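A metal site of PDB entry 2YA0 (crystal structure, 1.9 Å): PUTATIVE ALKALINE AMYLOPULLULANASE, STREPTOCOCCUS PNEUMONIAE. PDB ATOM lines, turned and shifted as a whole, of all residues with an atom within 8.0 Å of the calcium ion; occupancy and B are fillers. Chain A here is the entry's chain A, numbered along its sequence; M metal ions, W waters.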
ATOM      1  N   TYR A 205      -7.267  25.088  14.864  1.00  0.00           N
ATOM      2  CA  TYR A 205      -6.223  24.230  15.479  1.00  0.00           C
ATOM      3  C   TYR A 205      -4.838  24.548  14.913  1.00  0.00           C
ATOM      4  O   TYR A 205      -4.721  25.134  13.846  1.00  0.00           O
ATOM      5  CB  TYR A 205      -6.565  22.772  15.236  1.00  0.00           C
ATOM      6  CG  TYR A 205      -6.884  22.280  13.795  1.00  0.00           C
ATOM      7  CD1 TYR A 205      -5.854  21.920  12.863  1.00  0.00           C
ATOM      8  CD2 TYR A 205      -8.212  22.098  13.402  1.00  0.00           C
ATOM      9  CE1 TYR A 205      -6.183  21.440  11.636  1.00  0.00           C
ATOM     10  CE2 TYR A 205      -8.533  21.599  12.172  1.00  0.00           C
ATOM     11  CZ  TYR A 205      -7.490  21.284  11.266  1.00  0.00           C
ATOM     12  OH  TYR A 205      -7.898  20.744  10.090  1.00  0.00           O
ATOM     13  N   PHE A 207      -1.448  22.807  14.375  1.00  0.00           N
ATOM     14  CA  PHE A 207      -0.457  22.178  13.484  1.00  0.00           C
ATOM     15  C   PHE A 207      -1.051  21.879  12.134  1.00  0.00           C
ATOM     16  O   PHE A 207      -1.626  20.772  11.894  1.00  0.00           O
ATOM     17  CB  PHE A 207       0.187  20.931  14.125  1.00  0.00           C
ATOM     18  CG  PHE A 207       0.931  21.244  15.400  1.00  0.00           C
ATOM     19  CD1 PHE A 207       2.208  21.876  15.340  1.00  0.00           C
ATOM     20  CD2 PHE A 207       0.376  20.952  16.628  1.00  0.00           C
ATOM     21  CE1 PHE A 207       2.902  22.170  16.531  1.00  0.00           C
ATOM     22  CE2 PHE A 207       1.085  21.208  17.823  1.00  0.00           C
ATOM     23  CZ  PHE A 207       2.303  21.849  17.773  1.00  0.00           C
ATOM     24  N   VAL A 208      -0.907  22.866  11.225  1.00  0.00           N
ATOM     25  CA  VAL A 208      -1.489  22.698   9.904  1.00  0.00           C
ATOM     26  C   VAL A 208      -1.001  23.868   9.050  1.00  0.00           C
ATOM     27  O   VAL A 208      -0.651  24.912   9.589  1.00  0.00           O
ATOM     28  CB  VAL A 208      -3.023  22.783   9.997  1.00  0.00           C
ATOM     29  CG1 VAL A 208      -3.461  24.195  10.556  1.00  0.00           C
ATOM     30  CG2 VAL A 208      -3.601  22.464   8.685  1.00  0.00           C
ATOM     31  N   ASN A 209      -0.987  23.686   7.742  1.00  0.00           N
ATOM     32  CA  ASN A 209      -0.710  24.805   6.805  1.00  0.00           C
ATOM     33  C   ASN A 209      -1.932  24.970   5.978  1.00  0.00           C
ATOM     34  O   ASN A 209      -2.172  24.233   5.000  1.00  0.00           O
ATOM     35  CB  ASN A 209       0.474  24.513   5.906  1.00  0.00           C
ATOM     36  CG  ASN A 209       0.711  25.665   4.922  1.00  0.00           C
ATOM     37  OD1 ASN A 209      -0.065  26.648   4.918  1.00  0.00           O
ATOM     38  ND2 ASN A 209       1.735  25.551   4.084  1.00  0.00           N
ATOM     39  N   LEU A 217      -4.053  15.164  -0.741  1.00  0.00           N
ATOM     40  CA  LEU A 217      -3.018  14.417   0.000  1.00  0.00           C
ATOM     41  C   LEU A 217      -3.122  12.935  -0.422  1.00  0.00           C
ATOM     42  O   LEU A 217      -3.634  12.073   0.323  1.00  0.00           O
ATOM     43  CB  LEU A 217      -3.233  14.582   1.492  1.00  0.00           C
ATOM     44  CG  LEU A 217      -3.010  16.036   1.903  1.00  0.00           C
ATOM     45  CD1 LEU A 217      -3.544  16.292   3.319  1.00  0.00           C
ATOM     46  CD2 LEU A 217      -1.519  16.415   1.864  1.00  0.00           C
ATOM     47  N   SER A 222       1.169   8.104   7.095  1.00  0.00           N
ATOM     48  CA  SER A 222       0.462   8.076   8.406  1.00  0.00           C
ATOM     49  C   SER A 222       1.176   8.905   9.460  1.00  0.00           C
ATOM     50  O   SER A 222       0.843   8.828  10.632  1.00  0.00           O
ATOM     51  CB  SER A 222       0.239   6.660   8.879  1.00  0.00           C
ATOM     52  OG  SER A 222       1.509   5.924   8.911  1.00  0.00           O
ATOM     53  N   SER A 223       2.181   9.705   9.032  1.00  0.00           N
ATOM     54  CA  SER A 223       2.774  10.752   9.871  1.00  0.00           C
ATOM     55  C   SER A 223       3.245  11.886   8.991  1.00  0.00           C
ATOM     56  O   SER A 223       3.418  11.688   7.787  1.00  0.00           O
ATOM     57  CB  SER A 223       3.994  10.266  10.663  1.00  0.00           C
ATOM     58  OG  SER A 223       4.877   9.675   9.725  1.00  0.00           O
ATOM     59  N   ASN A 224       3.448  13.049   9.584  1.00  0.00           N
ATOM     60  CA  ASN A 224       3.984  14.227   8.904  1.00  0.00           C
ATOM     61  C   ASN A 224       3.115  14.561   7.675  1.00  0.00           C
ATOM     62  O   ASN A 224       3.613  14.784   6.558  1.00  0.00           O
ATOM     63  CB  ASN A 224       5.476  14.046   8.584  1.00  0.00           C
ATOM     64  CG  ASN A 224       6.176  15.321   8.073  1.00  0.00           C
ATOM     65  OD1 ASN A 224       5.888  16.446   8.536  1.00  0.00           O
ATOM     66  ND2 ASN A 224       7.134  15.152   7.115  1.00  0.00           N
ATOM     67  N   SER A 225       1.804  14.549   7.861  1.00  0.00           N
ATOM     68  CA  SER A 225       0.883  14.926   6.819  1.00  0.00           C
ATOM     69  C   SER A 225       0.273  16.299   7.157  1.00  0.00           C
ATOM     70  O   SER A 225       0.039  16.607   8.325  1.00  0.00           O
ATOM     71  CB  SER A 225      -0.255  13.931   6.762  1.00  0.00           C
ATOM     72  OG  SER A 225      -1.160  14.294   5.708  1.00  0.00           O
ATOM     73  N   ASN A 226      -0.077  17.082   6.146  1.00  0.00           N
ATOM     74  CA  ASN A 226      -0.737  18.340   6.456  1.00  0.00           C
ATOM     75  C   ASN A 226      -2.158  18.116   7.024  1.00  0.00           C
ATOM     76  O   ASN A 226      -2.722  19.051   7.695  1.00  0.00           O
ATOM     77  CB  ASN A 226      -0.761  19.269   5.232  1.00  0.00           C
ATOM     78  CG  ASN A 226      -1.152  20.681   5.601  1.00  0.00           C
ATOM     79  OD1 ASN A 226      -0.708  21.210   6.636  1.00  0.00           O
ATOM     80  ND2 ASN A 226      -1.953  21.320   4.740  1.00  0.00           N
ATOM     81  N   TYR A 227      -2.688  16.918   6.792  1.00  0.00           N
ATOM     82  CA  TYR A 227      -4.001  16.486   7.283  1.00  0.00           C
ATOM     83  C   TYR A 227      -3.939  16.557   8.850  1.00  0.00           C
ATOM     84  O   TYR A 227      -2.914  16.205   9.434  1.00  0.00           O
ATOM     85  CB  TYR A 227      -4.281  15.043   6.862  1.00  0.00           C
ATOM     86  CG  TYR A 227      -5.590  14.526   7.443  1.00  0.00           C
ATOM     87  CD1 TYR A 227      -5.659  14.064   8.790  1.00  0.00           C
ATOM     88  CD2 TYR A 227      -6.777  14.555   6.688  1.00  0.00           C
ATOM     89  CE1 TYR A 227      -6.906  13.584   9.357  1.00  0.00           C
ATOM     90  CE2 TYR A 227      -8.004  14.083   7.247  1.00  0.00           C
ATOM     91  CZ  TYR A 227      -8.035  13.607   8.573  1.00  0.00           C
ATOM     92  OH  TYR A 227      -9.264  13.156   9.054  1.00  0.00           O
ATOM     93  N   ASN A 228      -5.031  16.933   9.551  1.00  0.00           N
ATOM     94  CA  ASN A 228      -5.064  16.887  10.978  1.00  0.00           C
ATOM     95  C   ASN A 228      -6.516  16.638  11.390  1.00  0.00           C
ATOM     96  O   ASN A 228      -7.428  17.231  10.803  1.00  0.00           O
ATOM     97  CB  ASN A 228      -4.571  18.260  11.506  1.00  0.00           C
ATOM     98  CG  ASN A 228      -4.276  18.266  13.030  1.00  0.00           C
ATOM     99  OD1 ASN A 228      -4.888  17.542  13.822  1.00  0.00           O
ATOM    100  ND2 ASN A 228      -3.359  19.152  13.420  1.00  0.00           N
ATOM    101  N   TRP A 229      -6.756  15.729  12.327  1.00  0.00           N
ATOM    102  CA  TRP A 229      -8.111  15.585  12.898  1.00  0.00           C
ATOM    103  C   TRP A 229      -8.561  16.890  13.574  1.00  0.00           C
ATOM    104  O   TRP A 229      -9.785  17.211  13.627  1.00  0.00           O
ATOM    105  CB  TRP A 229      -8.060  14.498  14.000  1.00  0.00           C
ATOM    106  CG  TRP A 229      -8.282  13.144  13.492  1.00  0.00           C
ATOM    107  CD1 TRP A 229      -8.827  12.750  12.271  1.00  0.00           C
ATOM    108  CD2 TRP A 229      -8.045  11.928  14.237  1.00  0.00           C
ATOM    109  NE1 TRP A 229      -8.810  11.327  12.184  1.00  0.00           N
ATOM    110  CE2 TRP A 229      -8.350  10.835  13.379  1.00  0.00           C
ATOM    111  CE3 TRP A 229      -7.528  11.682  15.540  1.00  0.00           C
ATOM    112  CZ2 TRP A 229      -8.190   9.470  13.789  1.00  0.00           C
ATOM    113  CZ3 TRP A 229      -7.370  10.382  15.938  1.00  0.00           C
ATOM    114  CH2 TRP A 229      -7.739   9.286  15.078  1.00  0.00           C
ATOM    115  N   GLY A 230      -7.603  17.612  14.104  1.00  0.00           N
ATOM    116  CA  GLY A 230      -7.924  18.896  14.750  1.00  0.00           C
ATOM    117  C   GLY A 230      -7.841  18.983  16.259  1.00  0.00           C
ATOM    118  O   GLY A 230      -8.152  20.029  16.851  1.00  0.00           O
ATOM    119  N   ASP A 232      -5.548  19.887  18.293  1.00  0.00           N
ATOM    120  CA  ASP A 232      -4.424  20.732  18.714  1.00  0.00           C
ATOM    121  C   ASP A 232      -4.926  22.212  18.806  1.00  0.00           C
ATOM    122  O   ASP A 232      -4.641  23.027  17.897  1.00  0.00           O
ATOM    123  CB  ASP A 232      -3.243  20.673  17.676  1.00  0.00           C
ATOM    124  CG  ASP A 232      -2.773  19.311  17.417  1.00  0.00           C
ATOM    125  OD1 ASP A 232      -2.457  18.543  18.378  1.00  0.00           O
ATOM    126  OD2 ASP A 232      -2.591  19.025  16.250  1.00  0.00           O
ATOM    127  N   MET A 242      -8.914  25.549   7.442  1.00  0.00           N
ATOM    128  CA  MET A 242      -8.627  24.358   6.636  1.00  0.00           C
ATOM    129  C   MET A 242      -9.817  23.855   5.797  1.00  0.00           C
ATOM    130  O   MET A 242      -9.644  23.237   4.736  1.00  0.00           O
ATOM    131  CB  MET A 242      -8.113  23.314   7.655  1.00  0.00           C
ATOM    132  CG  MET A 242      -7.610  22.014   7.103  1.00  0.00           C
ATOM    133  SD  MET A 242      -6.176  22.366   6.008  1.00  0.00           S
ATOM    134  CE  MET A 242      -5.620  20.656   5.682  1.00  0.00           C
ATOM    135  N   SER A 554      -5.281   7.599  12.775  1.00  0.00           N
ATOM    136  CA  SER A 554      -5.093   8.346  11.521  1.00  0.00           C
ATOM    137  C   SER A 554      -5.105   9.881  11.674  1.00  0.00           C
ATOM    138  O   SER A 554      -5.278  10.592  10.668  1.00  0.00           O
ATOM    139  CB  SER A 554      -6.082   7.840  10.475  1.00  0.00           C
ATOM    140  OG  SER A 554      -7.383   8.156  10.839  1.00  0.00           O
ATOM    141  N   TYR A 555      -4.789  10.368  12.892  1.00  0.00           N
ATOM    142  CA  TYR A 555      -4.795  11.799  13.203  1.00  0.00           C
ATOM    143  C   TYR A 555      -3.844  12.638  12.305  1.00  0.00           C
ATOM    144  O   TYR A 555      -4.048  13.900  12.143  1.00  0.00           O
ATOM    145  CB  TYR A 555      -4.475  12.080  14.685  1.00  0.00           C
ATOM    146  CG  TYR A 555      -3.006  12.077  15.016  1.00  0.00           C
ATOM    147  CD1 TYR A 555      -2.237  10.870  14.979  1.00  0.00           C
ATOM    148  CD2 TYR A 555      -2.322  13.252  15.309  1.00  0.00           C
ATOM    149  CE1 TYR A 555      -0.875  10.872  15.277  1.00  0.00           C
ATOM    150  CE2 TYR A 555      -0.980  13.240  15.656  1.00  0.00           C
ATOM    151  CZ  TYR A 555      -0.252  12.027  15.626  1.00  0.00           C
ATOM    152  OH  TYR A 555       1.126  12.064  15.951  1.00  0.00           O
ATOM    153  N   ASP A 556      -2.846  11.978  11.754  1.00  0.00           N
ATOM    154  CA  ASP A 556      -1.727  12.620  11.055  1.00  0.00           C
ATOM    155  C   ASP A 556      -1.496  11.817   9.757  1.00  0.00           C
ATOM    156  O   ASP A 556      -0.329  11.648   9.279  1.00  0.00           O
ATOM    157  CB  ASP A 556      -0.505  12.709  12.008  1.00  0.00           C
ATOM    158  CG  ASP A 556       0.617  13.593  11.454  1.00  0.00           C
ATOM    159  OD1 ASP A 556       0.402  14.481  10.542  1.00  0.00           O
ATOM    160  OD2 ASP A 556       1.767  13.361  11.906  1.00  0.00           O
ATOM    161  N   SER A 557      -2.595  11.362   9.159  1.00  0.00           N
ATOM    162  CA  SER A 557      -2.528  10.550   7.937  1.00  0.00           C
ATOM    163  C   SER A 557      -3.132  11.228   6.713  1.00  0.00           C
ATOM    164  O   SER A 557      -4.055  12.054   6.885  1.00  0.00           O
ATOM    165  CB  SER A 557      -3.228   9.178   8.110  1.00  0.00           C
ATOM    166  OG  SER A 557      -2.560   8.381   9.117  1.00  0.00           O
ATOM    167  N   SER A 558      -2.708  10.827   5.496  1.00  0.00           N
ATOM    168  CA  SER A 558      -3.118  11.560   4.275  1.00  0.00           C
ATOM    169  C   SER A 558      -4.565  11.159   3.868  1.00  0.00           C
ATOM    170  O   SER A 558      -5.212  10.279   4.505  1.00  0.00           O
ATOM    171  CB  SER A 558      -2.124  11.221   3.152  1.00  0.00           C
ATOM    172  OG  SER A 558      -2.333   9.845   2.853  1.00  0.00           O
HETATM  173 CA    CA M   1      -0.802  16.571  10.550  1.00  0.00          CA
HETATM  174  O   HOH W   1       0.129  17.567  12.653  1.00  0.00           O
HETATM  175  O   HOH W   2      -2.040  15.843  12.477  1.00  0.00           O
HETATM  176  O   HOH W   3      -1.284  18.961  10.033  1.00  0.00           O
HETATM  177  O   HOH W   4       1.609  17.249  10.597  1.00  0.00           O
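Water W3 bridges O of Phe 207 (2.6 Å) and O of Asn 226 (2.7 Å).
The calcium ion is bound by O of Ser 225 (2.4 Å).
Water W2 is bound to the calcium ion, at 2.4 Å.
The calcium ion is bound by OD1 of Asp 556 (2.4 Å).
O of Tyr 227 is bound to the calcium ion (2.4 Å).
Water W3 binds the calcium ion, 2.5 Å away.
The calcium ion is bound by water W4, 2.5 Å away.
The calcium ion is bound by water W1 (2.5 Å).
The calcium ion has seven donor atoms within binding distance.
Of the 21 residues printed, 3 come within 4 Å of the calcium ion.
N of Asn 224 sits at hydrogen-bond distance from OD2 of Asp 556 (2.9 Å).
O of Asp 556 is in hydrogen-bond range of N of Ser 223, 3.2 Å away.
N of Tyr 227 sits close to OG of Ser 225 (3.2 Å).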
